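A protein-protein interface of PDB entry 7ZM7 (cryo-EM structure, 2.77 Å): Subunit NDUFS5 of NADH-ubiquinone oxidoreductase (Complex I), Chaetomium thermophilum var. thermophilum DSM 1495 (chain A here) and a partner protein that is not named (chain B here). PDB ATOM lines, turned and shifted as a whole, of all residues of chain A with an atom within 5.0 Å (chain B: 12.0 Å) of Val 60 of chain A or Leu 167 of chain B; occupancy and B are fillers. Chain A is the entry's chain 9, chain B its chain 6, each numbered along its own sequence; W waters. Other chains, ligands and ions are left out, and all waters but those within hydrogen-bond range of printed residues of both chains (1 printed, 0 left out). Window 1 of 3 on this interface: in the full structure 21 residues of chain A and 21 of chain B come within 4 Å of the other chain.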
ATOM      1  N   GLU A  56     -21.654  -3.992  27.885  1.00  0.00           N
ATOM      2  CA  GLU A  56     -20.544  -4.537  27.063  1.00  0.00           C
ATOM      3  C   GLU A  56     -21.033  -4.845  25.659  1.00  0.00           C
ATOM      4  O   GLU A  56     -20.286  -4.617  24.711  1.00  0.00           O
ATOM      5  CB  GLU A  56     -20.083  -5.862  27.636  1.00  0.00           C
ATOM      6  CG  GLU A  56     -18.616  -6.130  27.402  1.00  0.00           C
ATOM      7  CD  GLU A  56     -18.329  -7.604  27.212  1.00  0.00           C
ATOM      8  OE1 GLU A  56     -17.989  -8.266  28.202  1.00  0.00           O
ATOM      9  OE2 GLU A  56     -18.447  -8.078  26.073  1.00  0.00           O
ATOM     10  N   ALA A  57     -22.252  -5.338  25.541  1.00  0.00           N
ATOM     11  CA  ALA A  57     -22.834  -5.660  24.231  1.00  0.00           C
ATOM     12  C   ALA A  57     -23.012  -4.352  23.486  1.00  0.00           C
ATOM     13  O   ALA A  57     -22.717  -4.314  22.297  1.00  0.00           O
ATOM     14  CB  ALA A  57     -24.144  -6.354  24.429  1.00  0.00           C
ATOM     15  N   ALA A  58     -23.475  -3.321  24.194  1.00  0.00           N
ATOM     16  CA  ALA A  58     -23.614  -2.021  23.552  1.00  0.00           C
ATOM     17  C   ALA A  58     -22.269  -1.466  23.126  1.00  0.00           C
ATOM     18  O   ALA A  58     -22.135  -0.922  22.027  1.00  0.00           O
ATOM     19  CB  ALA A  58     -24.306  -1.049  24.496  1.00  0.00           C
ATOM     20  N   ARG A  59     -21.260  -1.593  23.981  1.00  0.00           N
ATOM     21  CA  ARG A  59     -19.940  -1.086  23.641  1.00  0.00           C
ATOM     22  C   ARG A  59     -19.331  -1.823  22.461  1.00  0.00           C
ATOM     23  O   ARG A  59     -18.861  -1.185  21.518  1.00  0.00           O
ATOM     24  CB  ARG A  59     -19.020  -1.182  24.847  1.00  0.00           C
ATOM     25  CG  ARG A  59     -17.620  -0.747  24.555  1.00  0.00           C
ATOM     26  CD  ARG A  59     -16.749  -0.955  25.745  1.00  0.00           C
ATOM     27  NE  ARG A  59     -15.356  -1.077  25.364  1.00  0.00           N
ATOM     28  CZ  ARG A  59     -14.805  -2.201  24.933  1.00  0.00           C
ATOM     29  NH1 ARG A  59     -15.542  -3.294  24.827  1.00  0.00           N
ATOM     30  NH2 ARG A  59     -13.522  -2.225  24.601  1.00  0.00           N
ATOM     31  N   VAL A  60     -19.344  -3.158  22.477  1.00  0.00           N
ATOM     32  CA  VAL A  60     -18.759  -3.937  21.393  1.00  0.00           C
ATOM     33  C   VAL A  60     -19.622  -3.918  20.140  1.00  0.00           C
ATOM     34  O   VAL A  60     -19.218  -4.467  19.110  1.00  0.00           O
ATOM     35  CB  VAL A  60     -18.461  -5.383  21.873  1.00  0.00           C
ATOM     36  CG1 VAL A  60     -17.610  -6.142  20.895  1.00  0.00           C
ATOM     37  CG2 VAL A  60     -17.709  -5.355  23.181  1.00  0.00           C
ATOM     38  N   ARG A  61     -20.779  -3.282  20.175  1.00  0.00           N
ATOM     39  CA  ARG A  61     -21.615  -3.211  18.986  1.00  0.00           C
ATOM     40  C   ARG A  61     -21.427  -1.917  18.217  1.00  0.00           C
ATOM     41  O   ARG A  61     -21.780  -1.851  17.039  1.00  0.00           O
ATOM     42  CB  ARG A  61     -23.087  -3.389  19.366  1.00  0.00           C
ATOM     43  CG  ARG A  61     -23.933  -3.961  18.278  1.00  0.00           C
ATOM     44  CD  ARG A  61     -25.390  -4.007  18.660  1.00  0.00           C
ATOM     45  NE  ARG A  61     -25.760  -5.242  19.344  1.00  0.00           N
ATOM     46  CZ  ARG A  61     -26.090  -5.316  20.629  1.00  0.00           C
ATOM     47  NH1 ARG A  61     -26.083  -4.233  21.392  1.00  0.00           N
ATOM     48  NH2 ARG A  61     -26.423  -6.482  21.157  1.00  0.00           N
ATOM     49  N   ALA A  62     -20.883  -0.888  18.864  1.00  0.00           N
ATOM     50  CA  ALA A  62     -20.452   0.316  18.168  1.00  0.00           C
ATOM     51  C   ALA A  62     -19.006   0.202  17.711  1.00  0.00           C
ATOM     52  O   ALA A  62     -18.663   0.622  16.605  1.00  0.00           O
ATOM     53  CB  ALA A  62     -20.615   1.524  19.073  1.00  0.00           C
ATOM     54  N   LEU A  63     -18.147  -0.365  18.555  1.00  0.00           N
ATOM     55  CA  LEU A  63     -16.739  -0.488  18.216  1.00  0.00           C
ATOM     56  C   LEU A  63     -16.578  -1.397  17.010  1.00  0.00           C
ATOM     57  O   LEU A  63     -15.673  -1.218  16.188  1.00  0.00           O
ATOM     58  CB  LEU A  63     -15.973  -1.055  19.406  1.00  0.00           C
ATOM     59  CG  LEU A  63     -14.437  -1.056  19.445  1.00  0.00           C
ATOM     60  CD1 LEU A  63     -13.980  -1.107  20.887  1.00  0.00           C
ATOM     61  CD2 LEU A  63     -13.721  -2.088  18.627  1.00  0.00           C
ATOM     62  N   GLN A  64     -17.441  -2.405  16.909  1.00  0.00           N
ATOM     63  CA  GLN A  64     -17.405  -3.311  15.775  1.00  0.00           C
ATOM     64  C   GLN A  64     -17.977  -2.664  14.530  1.00  0.00           C
ATOM     65  O   GLN A  64     -17.651  -3.075  13.417  1.00  0.00           O
ATOM     66  CB  GLN A  64     -18.160  -4.588  16.110  1.00  0.00           C
ATOM     67  CG  GLN A  64     -17.820  -5.761  15.230  1.00  0.00           C
ATOM     68  CD  GLN A  64     -18.920  -6.776  15.213  1.00  0.00           C
ATOM     69  OE1 GLN A  64     -20.078  -6.436  15.049  1.00  0.00           O
ATOM     70  NE2 GLN A  64     -18.568  -8.032  15.390  1.00  0.00           N
ATOM     71  N   LEU B   7      -6.788  -7.880  13.830  1.00  0.00           N
ATOM     72  CA  LEU B   7      -7.758  -8.945  14.183  1.00  0.00           C
ATOM     73  C   LEU B   7      -7.830  -9.919  13.013  1.00  0.00           C
ATOM     74  O   LEU B   7      -7.997  -9.448  11.885  1.00  0.00           O
ATOM     75  CB  LEU B   7      -9.122  -8.308  14.456  1.00  0.00           C
ATOM     76  CG  LEU B   7      -9.214  -7.408  15.683  1.00  0.00           C
ATOM     77  CD1 LEU B   7     -10.588  -6.759  15.751  1.00  0.00           C
ATOM     78  CD2 LEU B   7      -8.932  -8.198  16.952  1.00  0.00           C
ATOM     79  N   LEU B   9      -9.671 -13.570  11.603  1.00  0.00           N
ATOM     80  CA  LEU B   9     -10.767 -14.550  11.807  1.00  0.00           C
ATOM     81  C   LEU B   9     -10.567 -15.710  10.833  1.00  0.00           C
ATOM     82  O   LEU B   9     -10.483 -15.445   9.623  1.00  0.00           O
ATOM     83  CB  LEU B   9     -12.095 -13.843  11.527  1.00  0.00           C
ATOM     84  CG  LEU B   9     -13.355 -14.597  11.947  1.00  0.00           C
ATOM     85  CD1 LEU B   9     -13.334 -14.889  13.439  1.00  0.00           C
ATOM     86  CD2 LEU B   9     -14.597 -13.800  11.583  1.00  0.00           C
ATOM     87  N   HIS B  20     -25.040 -23.684  14.766  1.00  0.00           N
ATOM     88  CA  HIS B  20     -26.125 -23.087  15.573  1.00  0.00           C
ATOM     89  C   HIS B  20     -27.422 -23.208  14.781  1.00  0.00           C
ATOM     90  O   HIS B  20     -28.490 -22.894  15.333  1.00  0.00           O
ATOM     91  CB  HIS B  20     -25.810 -21.615  15.867  1.00  0.00           C
ATOM     92  CG  HIS B  20     -25.582 -20.792  14.646  1.00  0.00           C
ATOM     93  ND1 HIS B  20     -24.337 -20.668  14.063  1.00  0.00           N
ATOM     94  CD2 HIS B  20     -26.428 -20.051  13.899  1.00  0.00           C
ATOM     95  CE1 HIS B  20     -24.427 -19.888  13.006  1.00  0.00           C
ATOM     96  NE2 HIS B  20     -25.699 -19.496  12.884  1.00  0.00           N
ATOM     97  N   TYR B 127     -31.212 -10.126  29.159  1.00  0.00           N
ATOM     98  CA  TYR B 127     -30.519  -9.889  27.863  1.00  0.00           C
ATOM     99  C   TYR B 127     -29.887 -11.158  27.287  1.00  0.00           C
ATOM    100  O   TYR B 127     -29.945 -11.332  26.058  1.00  0.00           O
ATOM    101  CB  TYR B 127     -29.454  -8.806  27.992  1.00  0.00           C
ATOM    102  CG  TYR B 127     -29.191  -8.083  26.697  1.00  0.00           C
ATOM    103  CD1 TYR B 127     -30.186  -7.333  26.095  1.00  0.00           C
ATOM    104  CD2 TYR B 127     -27.957  -8.150  26.070  1.00  0.00           C
ATOM    105  CE1 TYR B 127     -29.964  -6.661  24.906  1.00  0.00           C
ATOM    106  CE2 TYR B 127     -27.720  -7.482  24.881  1.00  0.00           C
ATOM    107  CZ  TYR B 127     -28.726  -6.736  24.296  1.00  0.00           C
ATOM    108  OH  TYR B 127     -28.506  -6.075  23.123  1.00  0.00           O
ATOM    109  N   GLY B 128     -29.308 -12.011  28.128  1.00  0.00           N
ATOM    110  CA  GLY B 128     -28.613 -13.224  27.652  1.00  0.00           C
ATOM    111  C   GLY B 128     -29.534 -14.175  26.907  1.00  0.00           C
ATOM    112  O   GLY B 128     -29.038 -14.878  26.012  1.00  0.00           O
ATOM    113  N   VAL B 129     -30.815 -14.224  27.274  1.00  0.00           N
ATOM    114  CA  VAL B 129     -31.769 -15.195  26.656  1.00  0.00           C
ATOM    115  C   VAL B 129     -32.217 -14.674  25.285  1.00  0.00           C
ATOM    116  O   VAL B 129     -32.400 -15.505  24.375  1.00  0.00           O
ATOM    117  CB  VAL B 129     -32.967 -15.444  27.592  1.00  0.00           C
ATOM    118  CG1 VAL B 129     -34.114 -16.167  26.902  1.00  0.00           C
ATOM    119  CG2 VAL B 129     -32.540 -16.195  28.842  1.00  0.00           C
ATOM    120  N   ILE B 130     -32.328 -13.353  25.125  1.00  0.00           N
ATOM    121  CA  ILE B 130     -32.760 -12.771  23.857  1.00  0.00           C
ATOM    122  C   ILE B 130     -31.565 -12.231  23.082  1.00  0.00           C
ATOM    123  O   ILE B 130     -31.716 -11.361  22.218  1.00  0.00           O
ATOM    124  CB  ILE B 130     -33.808 -11.665  24.077  1.00  0.00           C
ATOM    125  CG1 ILE B 130     -33.236 -10.549  24.951  1.00  0.00           C
ATOM    126  CG2 ILE B 130     -35.064 -12.241  24.698  1.00  0.00           C
ATOM    127  CD1 ILE B 130     -34.148  -9.351  25.080  1.00  0.00           C
ATOM    128  N   ILE B 131     -30.368 -12.743  23.383  1.00  0.00           N
ATOM    129  CA  ILE B 131     -29.168 -12.299  22.680  1.00  0.00           C
ATOM    130  C   ILE B 131     -29.215 -12.652  21.199  1.00  0.00           C
ATOM    131  O   ILE B 131     -28.532 -12.011  20.392  1.00  0.00           O
ATOM    132  CB  ILE B 131     -27.913 -12.897  23.346  1.00  0.00           C
ATOM    133  CG1 ILE B 131     -26.659 -12.101  22.971  1.00  0.00           C
ATOM    134  CG2 ILE B 131     -27.751 -14.361  22.972  1.00  0.00           C
ATOM    135  CD1 ILE B 131     -26.697 -10.654  23.382  1.00  0.00           C
ATOM    136  N   SER B 132     -30.005 -13.651  20.818  1.00  0.00           N
ATOM    137  CA  SER B 132     -30.115 -14.055  19.421  1.00  0.00           C
ATOM    138  C   SER B 132     -31.504 -13.750  18.869  1.00  0.00           C
ATOM    139  O   SER B 132     -32.296 -14.659  18.614  1.00  0.00           O
ATOM    140  CB  SER B 132     -29.805 -15.545  19.270  1.00  0.00           C
ATOM    141  OG  SER B 132     -30.729 -16.338  19.997  1.00  0.00           O
ATOM    142  N   LYS B 164     -25.245  -6.077   8.441  1.00  0.00           N
ATOM    143  CA  LYS B 164     -25.610  -5.919   9.843  1.00  0.00           C
ATOM    144  C   LYS B 164     -24.543  -6.520  10.745  1.00  0.00           C
ATOM    145  O   LYS B 164     -24.211  -7.696  10.621  1.00  0.00           O
ATOM    146  CB  LYS B 164     -26.963  -6.574  10.120  1.00  0.00           C
ATOM    147  CG  LYS B 164     -27.190  -7.862   9.348  1.00  0.00           C
ATOM    148  CD  LYS B 164     -28.615  -8.360   9.506  1.00  0.00           C
ATOM    149  CE  LYS B 164     -28.859  -9.603   8.667  1.00  0.00           C
ATOM    150  NZ  LYS B 164     -30.241 -10.122   8.841  1.00  0.00           N
ATOM    151  N   ASN B 165     -24.005  -5.712  11.655  1.00  0.00           N
ATOM    152  CA  ASN B 165     -22.967  -6.183  12.566  1.00  0.00           C
ATOM    153  C   ASN B 165     -23.618  -7.055  13.629  1.00  0.00           C
ATOM    154  O   ASN B 165     -24.526  -6.612  14.339  1.00  0.00           O
ATOM    155  CB  ASN B 165     -22.221  -5.011  13.196  1.00  0.00           C
ATOM    156  CG  ASN B 165     -23.140  -4.057  13.918  1.00  0.00           C
ATOM    157  OD1 ASN B 165     -24.313  -3.926  13.570  1.00  0.00           O
ATOM    158  ND2 ASN B 165     -22.612  -3.376  14.925  1.00  0.00           N
ATOM    159  N   ASP B 166     -23.171  -8.298  13.731  1.00  0.00           N
ATOM    160  CA  ASP B 166     -23.663  -9.206  14.750  1.00  0.00           C
ATOM    161  C   ASP B 166     -22.590  -9.431  15.799  1.00  0.00           C
ATOM    162  O   ASP B 166     -21.416  -9.620  15.473  1.00  0.00           O
ATOM    163  CB  ASP B 166     -24.095 -10.543  14.146  1.00  0.00           C
ATOM    164  CG  ASP B 166     -25.541 -10.536  13.704  1.00  0.00           C
ATOM    165  OD1 ASP B 166     -26.258  -9.570  14.037  1.00  0.00           O
ATOM    166  OD2 ASP B 166     -25.964 -11.496  13.028  1.00  0.00           O
ATOM    167  N   LEU B 167     -22.998  -9.383  17.056  1.00  0.00           N
ATOM    168  CA  LEU B 167     -22.101  -9.684  18.147  1.00  0.00           C
ATOM    169  C   LEU B 167     -21.768 -11.160  18.156  1.00  0.00           C
ATOM    170  O   LEU B 167     -22.645 -12.019  18.059  1.00  0.00           O
ATOM    171  CB  LEU B 167     -22.731  -9.305  19.479  1.00  0.00           C
ATOM    172  CG  LEU B 167     -22.437  -7.933  20.058  1.00  0.00           C
ATOM    173  CD1 LEU B 167     -23.264  -7.783  21.302  1.00  0.00           C
ATOM    174  CD2 LEU B 167     -20.958  -7.773  20.354  1.00  0.00           C
ATOM    175  N   PHE B 168     -20.486 -11.447  18.301  1.00  0.00           N
ATOM    176  CA  PHE B 168     -19.990 -12.792  18.508  1.00  0.00           C
ATOM    177  C   PHE B 168     -19.571 -12.961  19.956  1.00  0.00           C
ATOM    178  O   PHE B 168     -18.931 -12.088  20.537  1.00  0.00           O
ATOM    179  CB  PHE B 168     -18.803 -13.087  17.592  1.00  0.00           C
ATOM    180  CG  PHE B 168     -19.187 -13.549  16.228  1.00  0.00           C
ATOM    181  CD1 PHE B 168     -19.381 -14.890  15.972  1.00  0.00           C
ATOM    182  CD2 PHE B 168     -19.301 -12.651  15.187  1.00  0.00           C
ATOM    183  CE1 PHE B 168     -19.721 -15.320  14.721  1.00  0.00           C
ATOM    184  CE2 PHE B 168     -19.636 -13.076  13.936  1.00  0.00           C
ATOM    185  CZ  PHE B 168     -19.846 -14.414  13.700  1.00  0.00           C
ATOM    186  N   PHE B 169     -19.909 -14.125  20.515  1.00  0.00           N
ATOM    187  CA  PHE B 169     -19.453 -14.472  21.884  1.00  0.00           C
ATOM    188  C   PHE B 169     -18.028 -15.008  21.760  1.00  0.00           C
ATOM    189  O   PHE B 169     -17.734 -15.690  20.775  1.00  0.00           O
ATOM    190  CB  PHE B 169     -20.341 -15.567  22.477  1.00  0.00           C
ATOM    191  CG  PHE B 169     -21.673 -15.094  22.993  1.00  0.00           C
ATOM    192  CD1 PHE B 169     -21.773 -14.488  24.234  1.00  0.00           C
ATOM    193  CD2 PHE B 169     -22.824 -15.268  22.246  1.00  0.00           C
ATOM    194  CE1 PHE B 169     -22.999 -14.061  24.716  1.00  0.00           C
ATOM    195  CE2 PHE B 169     -24.048 -14.839  22.728  1.00  0.00           C
ATOM    196  CZ  PHE B 169     -24.133 -14.239  23.962  1.00  0.00           C
ATOM    197  N   ILE B 170     -17.170 -14.694  22.724  1.00  0.00           N
ATOM    198  CA  ILE B 170     -15.743 -15.121  22.652  1.00  0.00           C
ATOM    199  C   ILE B 170     -15.422 -15.983  23.872  1.00  0.00           C
ATOM    200  O   ILE B 170     -15.957 -15.685  24.950  1.00  0.00           O
ATOM    201  CB  ILE B 170     -14.795 -13.907  22.506  1.00  0.00           C
ATOM    202  CG1 ILE B 170     -13.348 -14.323  22.232  1.00  0.00           C
ATOM    203  CG2 ILE B 170     -14.899 -12.957  23.688  1.00  0.00           C
ATOM    204  CD1 ILE B 170     -12.964 -14.282  20.780  1.00  0.00           C
ATOM    205  N   THR B 171     -14.618 -17.032  23.692  1.00  0.00           N
ATOM    206  CA  THR B 171     -14.181 -17.860  24.845  1.00  0.00           C
ATOM    207  C   THR B 171     -12.674 -18.122  24.788  1.00  0.00           C
ATOM    208  O   THR B 171     -12.131 -18.153  23.679  1.00  0.00           O
ATOM    209  CB  THR B 171     -14.974 -19.166  24.969  1.00  0.00           C
ATOM    210  OG1 THR B 171     -15.136 -19.747  23.676  1.00  0.00           O
ATOM    211  CG2 THR B 171     -16.313 -18.975  25.645  1.00  0.00           C
HETATM  212  O   HOH W   1     -18.628  -9.775  17.351  1.00  0.00           O
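The backbone carbonyl oxygen of Ala 57 of chain A lies close to the guanidinium group of Arg 61 of chain A, at 3.5 Å.
Among the printed residues, merely in contact across the chains: Ala 57 of chain A with Tyr 127 of chain B, Ala 57 of chain A with Leu 167 of chain B, Val 60 of chain A with Leu 167 of chain B, Arg 61 of chain A with Leu 167 of chain B and Gln 64 of chain A with Asn 165 of chain B.
Printed residues of chain A that touch a printed residue of chain B: Ala 57, Val 60, Arg 61 and Gln 64. Along chain A the printed residues that touch a printed residue of chain B span positions 57 to 64. Of the 17 printed residues of chain B, 4 touch a printed residue of chain A. Printed residues of chain B that touch a printed residue of chain A: Tyr 127, Asn 165, Asp 166 and Leu 167. Hydrophobic or aromatic side chains of chain B within 4 Å of the printed part of chain A: Tyr 127 and Leu 167.
Water W1 lies within hydrogen-bond range of NE2 of Gln 64 of chain A, N of Phe 168 of chain B and O of Asp 166 of chain B.
Of the printed residues of chain B, Val 60 of chain A touches Leu 167. Leu 167 of chain B touches just these residues of chain A: Ala 57 (3.5 Å), Val 60 (3.8 Å) and Arg 61 (3.4 Å). No residue of chain B comes within 4 Å of Glu 56 of chain A. Of the printed residues of chain B, Ala 57 of chain A touches Tyr 127 and Leu 167. No residue of chain B comes within 4 Å of Arg 59 of chain A. No residue of chain B comes within 4 Å of Leu 63 of chain A. Of the printed residues of chain A, Asp 166 of chain B touches Gln 64 (3.3 Å). Of the printed residues of chain A, Asn 165 of chain B touches Arg 61 and Gln 64. Of the printed residues of chain A, Tyr 127 of chain B touches Ala 57 (3.8 Å) and Arg 61 (2.9 Å). Gly 128 of chain B touches none of the printed residues of chain A. Phe 169 of chain B touches none of the printed residues of chain A. The nearest printed residue of chain A that does not touch Asn 165 of chain B is Ala 62 of chain A (5.0 Å).
NH2 of Arg 61 of chain A sits at hydrogen-bond distance from OH of Tyr 127 of chain B (2.9 Å). O of Arg 61 of chain A sits at hydrogen-bond distance from ND2 of Asn 165 of chain B, 2.7 Å away. The backbone carbonyl oxygen (O) of Asp 166 of chain B sits at hydrogen-bond distance from the side-chain amide nitrogen (NE2) of Gln 64 of chain A (3.3 Å).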
